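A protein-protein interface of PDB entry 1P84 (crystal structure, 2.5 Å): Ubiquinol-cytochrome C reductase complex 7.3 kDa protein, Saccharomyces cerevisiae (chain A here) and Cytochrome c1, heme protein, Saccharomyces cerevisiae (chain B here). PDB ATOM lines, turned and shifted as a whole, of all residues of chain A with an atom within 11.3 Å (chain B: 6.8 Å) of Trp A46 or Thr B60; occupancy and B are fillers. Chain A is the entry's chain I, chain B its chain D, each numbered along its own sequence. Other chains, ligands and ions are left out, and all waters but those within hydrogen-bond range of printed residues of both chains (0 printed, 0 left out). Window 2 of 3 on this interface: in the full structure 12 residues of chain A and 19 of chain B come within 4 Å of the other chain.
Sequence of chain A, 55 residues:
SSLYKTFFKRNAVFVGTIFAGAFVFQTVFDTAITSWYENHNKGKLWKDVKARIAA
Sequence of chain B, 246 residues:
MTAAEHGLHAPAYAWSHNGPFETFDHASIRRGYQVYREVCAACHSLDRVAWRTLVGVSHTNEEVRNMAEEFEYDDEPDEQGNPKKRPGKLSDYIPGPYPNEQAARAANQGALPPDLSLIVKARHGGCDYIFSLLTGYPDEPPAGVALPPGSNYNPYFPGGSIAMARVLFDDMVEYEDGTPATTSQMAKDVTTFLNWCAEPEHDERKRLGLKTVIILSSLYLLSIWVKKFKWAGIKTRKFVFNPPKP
The backbone carbonyl oxygen (O) of Lys A44 lies within hydrogen-bond range of the backbone NH (N) of His B26.
The backbone carbonyl oxygen (O) of Val B57 is in hydrogen-bond range of a ring nitrogen (ND1) of His B26, 2.8 Å away. The backbone carbonyl oxygen (O) of Ser B58 is in hydrogen-bond range of the guanidinium group (NH2) of Arg B30 (2.9 Å). The backbone NH (N) of His B59 is in hydrogen-bond range of the backbone carbonyl oxygen (O) of Leu B54, 3.4 Å away. A ring nitrogen (ND1) of His B59 lies within hydrogen-bond range of the side-chain hydroxyl (OG) of Ser B58, at 2.6 Å. The backbone NH (N) of Thr B60 is in hydrogen-bond range of the side-chain carboxylate (OE2) of Glu B63, at 3.0 Å. The side-chain amide oxygen (OD1) of Asn A41 sits at hydrogen-bond distance from the side-chain amino group (NZ) of Lys A44 (2.7 Å).
Among the printed residues, merely in contact across the chains: Trp A46 with Gly B56 (3.3 Å), Trp A46 with Ser B58 (3.4 Å), Trp A46 with Val B57 (3.5 Å), Trp A46 with His B59 (3.6 Å), Val A49 with Ala B27 (3.7 Å) and Trp A46 with Thr B60 (3.9 Å).
Trp A46 touches just these residues of chain B: Gly B56 (3.3 Å), Val B57 (3.5 Å), Ser B58 (3.4 Å), His B59 (3.6 Å) and Thr B60 (3.9 Å). Thr B60 touches one residue of chain A. Of chain A, only Lys A44 comes within 4 Å of His B26. No residue of chain A comes within 4 Å of Val B55. Gly B56 touches just one residue of chain A: Trp A46 (3.3 Å). Val B57 touches one residue of chain A. Printed residues of chain A within 4 Å of His B59: Trp A46. No residue of chain A comes within 4 Å of Asn B61. No residue of chain A comes within 4 Å of Glu B62. No residue of chain A comes within 4 Å of Glu B63. No residue of chain A comes within 4 Å of Val B64. Of the printed residues of chain A, Ala B27 touches Val A49 (3.7 Å). Of the printed residues of chain B, Val A49 touches Ala B27 (3.7 Å). Of the printed residues of chain B, Lys A44 touches His B26. Leu A45 touches none of the printed residues of chain B. The nearest printed residue of chain B that does not touch Lys A44 is Ala B27 (4.5 Å).
Printed residues of chain A that touch a printed residue of chain B: Lys A44, Trp A46 and Val A49. Hydrophobic or aromatic side chains of chain A that line the printed part of chain B: Trp A46 and Val A49. Hydrophobic or aromatic side chains of chain B within 4 Å of the printed part of chain A: His B26 and Ala B27. Among the printed residues, no Asp or Glu carboxylate lies within 4 Å of a Lys or Arg side-chain nitrogen of the other chain.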
ATOM      1  N   TYR A  37     -26.584  -6.200   1.460  1.00  0.00           N
ATOM      2  CA  TYR A  37     -25.446  -7.007   1.882  1.00  0.00           C
ATOM      3  C   TYR A  37     -24.859  -7.835   0.739  1.00  0.00           C
ATOM      4  O   TYR A  37     -23.653  -7.785   0.495  1.00  0.00           O
ATOM      5  CB  TYR A  37     -25.866  -7.914   3.054  1.00  0.00           C
ATOM      6  CG  TYR A  37     -24.735  -8.611   3.784  1.00  0.00           C
ATOM      7  CD1 TYR A  37     -23.828  -7.887   4.561  1.00  0.00           C
ATOM      8  CD2 TYR A  37     -24.591  -9.997   3.719  1.00  0.00           C
ATOM      9  CE1 TYR A  37     -22.802  -8.527   5.255  1.00  0.00           C
ATOM     10  CE2 TYR A  37     -23.575 -10.647   4.406  1.00  0.00           C
ATOM     11  CZ  TYR A  37     -22.684  -9.907   5.173  1.00  0.00           C
ATOM     12  OH  TYR A  37     -21.686 -10.547   5.862  1.00  0.00           O
ATOM     13  N   GLU A  38     -25.707  -8.595   0.046  1.00  0.00           N
ATOM     14  CA  GLU A  38     -25.252  -9.429  -1.074  1.00  0.00           C
ATOM     15  C   GLU A  38     -24.700  -8.610  -2.241  1.00  0.00           C
ATOM     16  O   GLU A  38     -23.760  -9.032  -2.915  1.00  0.00           O
ATOM     17  CB  GLU A  38     -26.373 -10.349  -1.568  1.00  0.00           C
ATOM     18  CG  GLU A  38     -26.634 -11.543  -0.670  1.00  0.00           C
ATOM     19  CD  GLU A  38     -27.649 -12.516  -1.249  1.00  0.00           C
ATOM     20  OE1 GLU A  38     -27.741 -13.650  -0.725  1.00  0.00           O
ATOM     21  OE2 GLU A  38     -28.356 -12.158  -2.222  1.00  0.00           O
ATOM     22  N   ASN A  39     -25.279  -7.439  -2.471  1.00  0.00           N
ATOM     23  CA  ASN A  39     -24.829  -6.575  -3.549  1.00  0.00           C
ATOM     24  C   ASN A  39     -23.447  -6.010  -3.222  1.00  0.00           C
ATOM     25  O   ASN A  39     -22.588  -5.902  -4.100  1.00  0.00           O
ATOM     26  CB  ASN A  39     -25.829  -5.436  -3.783  1.00  0.00           C
ATOM     27  CG  ASN A  39     -25.444  -4.558  -4.965  1.00  0.00           C
ATOM     28  OD1 ASN A  39     -25.663  -4.923  -6.125  1.00  0.00           O
ATOM     29  ND2 ASN A  39     -24.838  -3.409  -4.678  1.00  0.00           N
ATOM     30  N   ASN A  41     -21.167  -7.411  -1.508  1.00  0.00           N
ATOM     31  CA  ASN A  41     -20.180  -8.474  -1.643  1.00  0.00           C
ATOM     32  C   ASN A  41     -20.264  -9.244  -2.958  1.00  0.00           C
ATOM     33  O   ASN A  41     -19.831 -10.390  -3.039  1.00  0.00           O
ATOM     34  CB  ASN A  41     -20.267  -9.440  -0.457  1.00  0.00           C
ATOM     35  CG  ASN A  41     -19.710  -8.842   0.825  1.00  0.00           C
ATOM     36  OD1 ASN A  41     -18.525  -9.004   1.136  1.00  0.00           O
ATOM     37  ND2 ASN A  41     -20.564  -8.146   1.579  1.00  0.00           N
ATOM     38  N   LYS A  42     -20.800  -8.600  -3.990  1.00  0.00           N
ATOM     39  CA  LYS A  42     -20.923  -9.223  -5.308  1.00  0.00           C
ATOM     40  C   LYS A  42     -19.544  -9.650  -5.817  1.00  0.00           C
ATOM     41  O   LYS A  42     -18.587  -8.880  -5.774  1.00  0.00           O
ATOM     42  CB  LYS A  42     -21.562  -8.253  -6.308  1.00  0.00           C
ATOM     43  CG  LYS A  42     -22.043  -8.929  -7.595  1.00  0.00           C
ATOM     44  CD  LYS A  42     -22.455  -7.916  -8.664  1.00  0.00           C
ATOM     45  CE  LYS A  42     -23.656  -7.059  -8.235  1.00  0.00           C
ATOM     46  NZ  LYS A  42     -24.924  -7.848  -8.062  1.00  0.00           N
ATOM     47  N   GLY A  43     -19.453 -10.896  -6.266  1.00  0.00           N
ATOM     48  CA  GLY A  43     -18.200 -11.421  -6.768  1.00  0.00           C
ATOM     49  C   GLY A  43     -17.503 -12.334  -5.778  1.00  0.00           C
ATOM     50  O   GLY A  43     -16.715 -13.189  -6.180  1.00  0.00           O
ATOM     51  N   LYS A  44     -17.814 -12.172  -4.490  1.00  0.00           N
ATOM     52  CA  LYS A  44     -17.198 -12.965  -3.426  1.00  0.00           C
ATOM     53  C   LYS A  44     -18.026 -14.155  -2.966  1.00  0.00           C
ATOM     54  O   LYS A  44     -17.473 -15.148  -2.478  1.00  0.00           O
ATOM     55  CB  LYS A  44     -16.866 -12.066  -2.233  1.00  0.00           C
ATOM     56  CG  LYS A  44     -15.688 -11.132  -2.473  1.00  0.00           C
ATOM     57  CD  LYS A  44     -15.763  -9.859  -1.625  1.00  0.00           C
ATOM     58  CE  LYS A  44     -15.683 -10.144  -0.136  1.00  0.00           C
ATOM     59  NZ  LYS A  44     -15.825  -8.895   0.660  1.00  0.00           N
ATOM     60  N   LEU A  45     -19.343 -14.057  -3.140  1.00  0.00           N
ATOM     61  CA  LEU A  45     -20.287 -15.110  -2.742  1.00  0.00           C
ATOM     62  C   LEU A  45     -20.199 -16.406  -3.540  1.00  0.00           C
ATOM     63  O   LEU A  45     -19.627 -16.448  -4.626  1.00  0.00           O
ATOM     64  CB  LEU A  45     -21.721 -14.589  -2.835  1.00  0.00           C
ATOM     65  CG  LEU A  45     -22.322 -13.727  -1.726  1.00  0.00           C
ATOM     66  CD1 LEU A  45     -21.252 -13.082  -0.862  1.00  0.00           C
ATOM     67  CD2 LEU A  45     -23.228 -12.675  -2.352  1.00  0.00           C
ATOM     68  N   TRP A  46     -20.797 -17.458  -2.991  1.00  0.00           N
ATOM     69  CA  TRP A  46     -20.846 -18.768  -3.637  1.00  0.00           C
ATOM     70  C   TRP A  46     -21.713 -18.695  -4.892  1.00  0.00           C
ATOM     71  O   TRP A  46     -21.439 -19.383  -5.867  1.00  0.00           O
ATOM     72  CB  TRP A  46     -21.424 -19.821  -2.687  1.00  0.00           C
ATOM     73  CG  TRP A  46     -21.691 -21.153  -3.344  1.00  0.00           C
ATOM     74  CD1 TRP A  46     -22.900 -21.783  -3.463  1.00  0.00           C
ATOM     75  CD2 TRP A  46     -20.726 -22.022  -3.952  1.00  0.00           C
ATOM     76  NE1 TRP A  46     -22.745 -22.992  -4.099  1.00  0.00           N
ATOM     77  CE2 TRP A  46     -21.422 -23.165  -4.410  1.00  0.00           C
ATOM     78  CE3 TRP A  46     -19.341 -21.951  -4.152  1.00  0.00           C
ATOM     79  CZ2 TRP A  46     -20.780 -24.228  -5.053  1.00  0.00           C
ATOM     80  CZ3 TRP A  46     -18.700 -23.008  -4.793  1.00  0.00           C
ATOM     81  CH2 TRP A  46     -19.423 -24.132  -5.234  1.00  0.00           C
ATOM     82  N   LYS A  47     -22.780 -17.894  -4.838  1.00  0.00           N
ATOM     83  CA  LYS A  47     -23.678 -17.714  -5.974  1.00  0.00           C
ATOM     84  C   LYS A  47     -22.824 -17.298  -7.157  1.00  0.00           C
ATOM     85  O   LYS A  47     -22.851 -17.924  -8.214  1.00  0.00           O
ATOM     86  CB  LYS A  47     -24.685 -16.587  -5.723  1.00  0.00           C
ATOM     87  CG  LYS A  47     -25.537 -16.718  -4.481  1.00  0.00           C
ATOM     88  CD  LYS A  47     -26.649 -15.670  -4.482  1.00  0.00           C
ATOM     89  CE  LYS A  47     -26.109 -14.257  -4.694  1.00  0.00           C
ATOM     90  NZ  LYS A  47     -27.201 -13.231  -4.706  1.00  0.00           N
ATOM     91  N   ASP A  48     -22.031 -16.253  -6.938  1.00  0.00           N
ATOM     92  CA  ASP A  48     -21.153 -15.702  -7.954  1.00  0.00           C
ATOM     93  C   ASP A  48     -20.074 -16.681  -8.406  1.00  0.00           C
ATOM     94  O   ASP A  48     -19.731 -16.728  -9.583  1.00  0.00           O
ATOM     95  CB  ASP A  48     -20.528 -14.403  -7.439  1.00  0.00           C
ATOM     96  CG  ASP A  48     -21.572 -13.426  -6.904  1.00  0.00           C
ATOM     97  OD1 ASP A  48     -21.280 -12.717  -5.919  1.00  0.00           O
ATOM     98  OD2 ASP A  48     -22.693 -13.375  -7.453  1.00  0.00           O
ATOM     99  N   VAL A  49     -19.554 -17.472  -7.477  1.00  0.00           N
ATOM    100  CA  VAL A  49     -18.520 -18.451  -7.802  1.00  0.00           C
ATOM    101  C   VAL A  49     -19.094 -19.646  -8.566  1.00  0.00           C
ATOM    102  O   VAL A  49     -18.441 -20.183  -9.456  1.00  0.00           O
ATOM    103  CB  VAL A  49     -17.782 -18.937  -6.520  1.00  0.00           C
ATOM    104  CG1 VAL A  49     -16.854 -20.104  -6.830  1.00  0.00           C
ATOM    105  CG2 VAL A  49     -16.985 -17.793  -5.921  1.00  0.00           C
ATOM    106  N   LYS A  50     -20.322 -20.036  -8.235  1.00  0.00           N
ATOM    107  CA  LYS A  50     -20.988 -21.168  -8.882  1.00  0.00           C
ATOM    108  C   LYS A  50     -21.203 -20.924 -10.373  1.00  0.00           C
ATOM    109  O   LYS A  50     -21.159 -21.859 -11.174  1.00  0.00           O
ATOM    110  CB  LYS A  50     -22.332 -21.455  -8.204  1.00  0.00           C
ATOM    111  CG  LYS A  50     -23.023 -22.723  -8.680  1.00  0.00           C
ATOM    112  CD  LYS A  50     -24.368 -22.915  -7.989  1.00  0.00           C
ATOM    113  CE  LYS A  50     -24.980 -24.266  -8.338  1.00  0.00           C
ATOM    114  NZ  LYS A  50     -26.258 -24.510  -7.604  1.00  0.00           N
ATOM    115  N   ALA A  51     -21.444 -19.667 -10.738  1.00  0.00           N
ATOM    116  CA  ALA A  51     -21.659 -19.289 -12.132  1.00  0.00           C
ATOM    117  C   ALA A  51     -20.373 -19.447 -12.948  1.00  0.00           C
ATOM    118  O   ALA A  51     -20.403 -19.923 -14.085  1.00  0.00           O
ATOM    119  CB  ALA A  51     -22.168 -17.853 -12.217  1.00  0.00           C
ATOM    120  N   ARG A  52     -19.244 -19.071 -12.350  1.00  0.00           N
ATOM    121  CA  ARG A  52     -17.937 -19.161 -13.003  1.00  0.00           C
ATOM    122  C   ARG A  52     -17.432 -20.603 -13.050  1.00  0.00           C
ATOM    123  O   ARG A  52     -16.317 -20.866 -13.501  1.00  0.00           O
ATOM    124  CB  ARG A  52     -16.916 -18.290 -12.269  1.00  0.00           C
ATOM    125  CG  ARG A  52     -17.427 -16.903 -11.894  1.00  0.00           C
ATOM    126  CD  ARG A  52     -16.492 -15.813 -12.386  1.00  0.00           C
ATOM    127  NE  ARG A  52     -16.519 -15.691 -13.844  1.00  0.00           N
ATOM    128  CZ  ARG A  52     -15.441 -15.567 -14.613  1.00  0.00           C
ATOM    129  NH1 ARG A  52     -14.228 -15.549 -14.072  1.00  0.00           N
ATOM    130  NH2 ARG A  52     -15.577 -15.462 -15.928  1.00  0.00           N
ATOM    131  N   ILE A  53     -18.250 -21.523 -12.547  1.00  0.00           N
ATOM    132  CA  ILE A  53     -17.917 -22.943 -12.522  1.00  0.00           C
ATOM    133  C   ILE A  53     -18.882 -23.686 -13.448  1.00  0.00           C
ATOM    134  O   ILE A  53     -20.049 -23.306 -13.574  1.00  0.00           O
ATOM    135  CB  ILE A  53     -18.025 -23.523 -11.080  1.00  0.00           C
ATOM    136  CG1 ILE A  53     -17.079 -22.775 -10.132  1.00  0.00           C
ATOM    137  CG2 ILE A  53     -17.715 -25.018 -11.067  1.00  0.00           C
ATOM    138  CD1 ILE A  53     -15.617 -22.794 -10.552  1.00  0.00           C
ATOM    139  N   ALA A  54     -18.385 -24.729 -14.106  1.00  0.00           N
ATOM    140  CA  ALA A  54     -19.201 -25.526 -15.019  1.00  0.00           C
ATOM    141  C   ALA A  54     -18.834 -27.008 -14.928  1.00  0.00           C
ATOM    142  O   ALA A  54     -17.807 -27.442 -15.458  1.00  0.00           O
ATOM    143  CB  ALA A  54     -19.040 -25.020 -16.455  1.00  0.00           C
ATOM    144  N   ALA A  55     -19.687 -27.774 -14.253  1.00  0.00           N
ATOM    145  CA  ALA A  55     -19.475 -29.209 -14.072  1.00  0.00           C
ATOM    146  C   ALA A  55     -20.802 -29.966 -13.987  1.00  0.00           C
ATOM    147  O   ALA A  55     -20.759 -31.212 -13.873  1.00  0.00           O
ATOM    148  CB  ALA A  55     -18.633 -29.462 -12.814  1.00  0.00           C
ATOM    149  OXT ALA A  55     -21.870 -29.314 -14.043  1.00  0.00           O
ATOM    150  N   HIS B  26     -15.325 -16.653  -1.350  1.00  0.00           N
ATOM    151  CA  HIS B  26     -15.496 -18.093  -1.514  1.00  0.00           C
ATOM    152  C   HIS B  26     -14.645 -18.777  -2.582  1.00  0.00           C
ATOM    153  O   HIS B  26     -14.403 -19.986  -2.507  1.00  0.00           O
ATOM    154  CB  HIS B  26     -16.974 -18.439  -1.635  1.00  0.00           C
ATOM    155  CG  HIS B  26     -17.746 -18.165  -0.380  1.00  0.00           C
ATOM    156  ND1 HIS B  26     -18.320 -19.163   0.377  1.00  0.00           N
ATOM    157  CD2 HIS B  26     -17.999 -17.004   0.275  1.00  0.00           C
ATOM    158  CE1 HIS B  26     -18.890 -18.630   1.444  1.00  0.00           C
ATOM    159  NE2 HIS B  26     -18.709 -17.322   1.405  1.00  0.00           N
ATOM    160  N   ALA B  27     -14.160 -18.001  -3.549  1.00  0.00           N
ATOM    161  CA  ALA B  27     -13.299 -18.543  -4.596  1.00  0.00           C
ATOM    162  C   ALA B  27     -11.972 -18.878  -3.926  1.00  0.00           C
ATOM    163  O   ALA B  27     -11.386 -19.942  -4.157  1.00  0.00           O
ATOM    164  CB  ALA B  27     -13.093 -17.519  -5.699  1.00  0.00           C
ATOM    165  N   ARG B  30     -12.265 -21.983  -1.846  1.00  0.00           N
ATOM    166  CA  ARG B  30     -12.186 -23.137  -2.760  1.00  0.00           C
ATOM    167  C   ARG B  30     -10.737 -23.516  -3.079  1.00  0.00           C
ATOM    168  O   ARG B  30     -10.332 -24.668  -2.884  1.00  0.00           O
ATOM    169  CB  ARG B  30     -12.945 -22.837  -4.060  1.00  0.00           C
ATOM    170  CG  ARG B  30     -13.012 -23.998  -5.054  1.00  0.00           C
ATOM    171  CD  ARG B  30     -13.989 -23.665  -6.186  1.00  0.00           C
ATOM    172  NE  ARG B  30     -13.989 -24.651  -7.266  1.00  0.00           N
ATOM    173  CZ  ARG B  30     -14.713 -25.767  -7.274  1.00  0.00           C
ATOM    174  NH1 ARG B  30     -14.642 -26.589  -8.311  1.00  0.00           N
ATOM    175  NH2 ARG B  30     -15.502 -26.075  -6.253  1.00  0.00           N
ATOM    176  N   LEU B  54     -18.908 -28.153   3.560  1.00  0.00           N
ATOM    177  CA  LEU B  54     -18.282 -27.639   2.340  1.00  0.00           C
ATOM    178  C   LEU B  54     -19.328 -27.325   1.264  1.00  0.00           C
ATOM    179  O   LEU B  54     -19.179 -26.369   0.498  1.00  0.00           O
ATOM    180  CB  LEU B  54     -17.244 -28.620   1.800  1.00  0.00           C
ATOM    181  CG  LEU B  54     -15.785 -28.239   2.095  1.00  0.00           C
ATOM    182  CD1 LEU B  54     -15.510 -28.358   3.587  1.00  0.00           C
ATOM    183  CD2 LEU B  54     -14.835 -29.140   1.311  1.00  0.00           C
ATOM    184  N   VAL B  55     -20.410 -28.102   1.251  1.00  0.00           N
ATOM    185  CA  VAL B  55     -21.493 -27.919   0.286  1.00  0.00           C
ATOM    186  C   VAL B  55     -22.132 -26.539   0.373  1.00  0.00           C
ATOM    187  O   VAL B  55     -22.627 -26.135   1.428  1.00  0.00           O
ATOM    188  CB  VAL B  55     -22.597 -28.963   0.481  1.00  0.00           C
ATOM    189  CG1 VAL B  55     -23.770 -28.664  -0.439  1.00  0.00           C
ATOM    190  CG2 VAL B  55     -22.043 -30.354   0.240  1.00  0.00           C
ATOM    191  N   GLY B  56     -22.137 -25.834  -0.750  1.00  0.00           N
ATOM    192  CA  GLY B  56     -22.728 -24.512  -0.787  1.00  0.00           C
ATOM    193  C   GLY B  56     -21.793 -23.434  -0.297  1.00  0.00           C
ATOM    194  O   GLY B  56     -22.171 -22.261  -0.263  1.00  0.00           O
ATOM    195  N   VAL B  57     -20.575 -23.822   0.085  1.00  0.00           N
ATOM    196  CA  VAL B  57     -19.595 -22.860   0.578  1.00  0.00           C
ATOM    197  C   VAL B  57     -18.438 -22.733  -0.391  1.00  0.00           C
ATOM    198  O   VAL B  57     -18.118 -21.634  -0.846  1.00  0.00           O
ATOM    199  CB  VAL B  57     -19.031 -23.257   1.976  1.00  0.00           C
ATOM    200  CG1 VAL B  57     -17.946 -22.266   2.415  1.00  0.00           C
ATOM    201  CG2 VAL B  57     -20.152 -23.304   3.008  1.00  0.00           C
ATOM    202  N   SER B  58     -17.823 -23.867  -0.706  1.00  0.00           N
ATOM    203  CA  SER B  58     -16.683 -23.892  -1.611  1.00  0.00           C
ATOM    204  C   SER B  58     -16.798 -24.967  -2.708  1.00  0.00           C
ATOM    205  O   SER B  58     -15.992 -25.000  -3.639  1.00  0.00           O
ATOM    206  CB  SER B  58     -15.415 -24.145  -0.804  1.00  0.00           C
ATOM    207  OG  SER B  58     -15.471 -25.421  -0.197  1.00  0.00           O
ATOM    208  N   HIS B  59     -17.767 -25.866  -2.566  1.00  0.00           N
ATOM    209  CA  HIS B  59     -17.969 -26.951  -3.519  1.00  0.00           C
ATOM    210  C   HIS B  59     -19.441 -27.325  -3.621  1.00  0.00           C
ATOM    211  O   HIS B  59     -20.235 -26.995  -2.741  1.00  0.00           O
ATOM    212  CB  HIS B  59     -17.177 -28.184  -3.084  1.00  0.00           C
ATOM    213  CG  HIS B  59     -15.696 -27.974  -3.054  1.00  0.00           C
ATOM    214  ND1 HIS B  59     -15.073 -27.205  -2.095  1.00  0.00           N
ATOM    215  CD2 HIS B  59     -14.713 -28.441  -3.856  1.00  0.00           C
ATOM    216  CE1 HIS B  59     -13.771 -27.209  -2.309  1.00  0.00           C
ATOM    217  NE2 HIS B  59     -13.526 -27.953  -3.371  1.00  0.00           N
ATOM    218  N   THR B  60     -19.803 -28.011  -4.702  1.00  0.00           N
ATOM    219  CA  THR B  60     -21.184 -28.437  -4.904  1.00  0.00           C
ATOM    220  C   THR B  60     -21.444 -29.710  -4.118  1.00  0.00           C
ATOM    221  O   THR B  60     -20.514 -30.403  -3.691  1.00  0.00           O
ATOM    222  CB  THR B  60     -21.504 -28.727  -6.389  1.00  0.00           C
ATOM    223  OG1 THR B  60     -20.725 -29.845  -6.837  1.00  0.00           O
ATOM    224  CG2 THR B  60     -21.212 -27.514  -7.255  1.00  0.00           C
ATOM    225  N   ASN B  61     -22.722 -30.034  -3.973  1.00  0.00           N
ATOM    226  CA  ASN B  61     -23.137 -31.223  -3.253  1.00  0.00           C
ATOM    227  C   ASN B  61     -22.484 -32.458  -3.872  1.00  0.00           C
ATOM    228  O   ASN B  61     -21.989 -33.335  -3.165  1.00  0.00           O
ATOM    229  CB  ASN B  61     -24.659 -31.340  -3.305  1.00  0.00           C
ATOM    230  CG  ASN B  61     -25.192 -32.372  -2.343  1.00  0.00           C
ATOM    231  OD1 ASN B  61     -25.017 -33.575  -2.545  1.00  0.00           O
ATOM    232  ND2 ASN B  61     -25.834 -31.908  -1.275  1.00  0.00           N
ATOM    233  N   GLU B  62     -22.454 -32.488  -5.201  1.00  0.00           N
ATOM    234  CA  GLU B  62     -21.870 -33.595  -5.953  1.00  0.00           C
ATOM    235  C   GLU B  62     -20.367 -33.716  -5.718  1.00  0.00           C
ATOM    236  O   GLU B  62     -19.874 -34.800  -5.391  1.00  0.00           O
ATOM    237  CB  GLU B  62     -22.146 -33.435  -7.456  1.00  0.00           C
ATOM    238  CG  GLU B  62     -23.615 -33.602  -7.875  1.00  0.00           C
ATOM    239  CD  GLU B  62     -24.530 -32.476  -7.390  1.00  0.00           C
ATOM    240  OE1 GLU B  62     -24.176 -31.286  -7.571  1.00  0.00           O
ATOM    241  OE2 GLU B  62     -25.612 -32.788  -6.836  1.00  0.00           O
ATOM    242  N   GLU B  63     -19.649 -32.600  -5.875  1.00  0.00           N
ATOM    243  CA  GLU B  63     -18.194 -32.570  -5.686  1.00  0.00           C
ATOM    244  C   GLU B  63     -17.757 -33.094  -4.326  1.00  0.00           C
ATOM    245  O   GLU B  63     -16.795 -33.858  -4.232  1.00  0.00           O
ATOM    246  CB  GLU B  63     -17.650 -31.156  -5.852  1.00  0.00           C
ATOM    247  CG  GLU B  63     -17.821 -30.562  -7.223  1.00  0.00           C
ATOM    248  CD  GLU B  63     -17.201 -29.185  -7.323  1.00  0.00           C
ATOM    249  OE1 GLU B  63     -16.000 -29.101  -7.660  1.00  0.00           O
ATOM    250  OE2 GLU B  63     -17.911 -28.192  -7.051  1.00  0.00           O
ATOM    251  N   VAL B  64     -18.457 -32.670  -3.275  1.00  0.00           N
ATOM    252  CA  VAL B  64     -18.125 -33.101  -1.925  1.00  0.00           C
ATOM    253  C   VAL B  64     -18.396 -34.589  -1.748  1.00  0.00           C
ATOM    254  O   VAL B  64     -17.639 -35.288  -1.069  1.00  0.00           O
ATOM    255  CB  VAL B  64     -18.908 -32.301  -0.857  1.00  0.00           C
ATOM    256  CG1 VAL B  64     -18.541 -32.779   0.537  1.00  0.00           C
ATOM    257  CG2 VAL B  64     -18.609 -30.821  -0.992  1.00  0.00           C
ATOM    258  N   ARG B  65     -19.466 -35.074  -2.375  1.00  0.00           N
ATOM    259  CA  ARG B  65     -19.824 -36.483  -2.278  1.00  0.00           C
ATOM    260  C   ARG B  65     -18.716 -37.342  -2.882  1.00  0.00           C
ATOM    261  O   ARG B  65     -18.322 -38.349  -2.296  1.00  0.00           O
ATOM    262  CB  ARG B  65     -21.175 -36.751  -2.954  1.00  0.00           C
ATOM    263  CG  ARG B  65     -21.690 -38.186  -2.788  1.00  0.00           C
ATOM    264  CD  ARG B  65     -23.131 -38.346  -3.270  1.00  0.00           C
ATOM    265  NE  ARG B  65     -24.108 -38.025  -2.224  1.00  0.00           N
ATOM    266  CZ  ARG B  65     -25.036 -37.072  -2.317  1.00  0.00           C
ATOM    267  NH1 ARG B  65     -25.881 -36.866  -1.313  1.00  0.00           N
ATOM    268  NH2 ARG B  65     -25.109 -36.314  -3.405  1.00  0.00           N
ATOM    269  N   MET B  67     -15.523 -36.480  -3.230  1.00  0.00           N
ATOM    270  CA  MET B  67     -14.352 -36.330  -2.369  1.00  0.00           C
ATOM    271  C   MET B  67     -14.399 -37.202  -1.125  1.00  0.00           C
ATOM    272  O   MET B  67     -13.391 -37.804  -0.743  1.00  0.00           O
ATOM    273  CB  MET B  67     -14.179 -34.876  -1.942  1.00  0.00           C
ATOM    274  CG  MET B  67     -13.653 -33.964  -3.025  1.00  0.00           C
ATOM    275  SD  MET B  67     -13.208 -32.356  -2.355  1.00  0.00           S
ATOM    276  CE  MET B  67     -14.758 -31.490  -2.516  1.00  0.00           C
ATOM    277  N   LEU B  90     -21.485 -37.626   3.372  1.00  0.00           N
ATOM    278  CA  LEU B  90     -21.477 -36.233   3.804  1.00  0.00           C
ATOM    279  C   LEU B  90     -21.460 -36.013   5.318  1.00  0.00           C
ATOM    280  O   LEU B  90     -20.861 -35.047   5.800  1.00  0.00           O
ATOM    281  CB  LEU B  90     -22.632 -35.459   3.168  1.00  0.00           C
ATOM    282  CG  LEU B  90     -22.592 -35.309   1.642  1.00  0.00           C
ATOM    283  CD1 LEU B  90     -23.634 -34.286   1.181  1.00  0.00           C
ATOM    284  CD2 LEU B  90     -21.213 -34.877   1.198  1.00  0.00           C
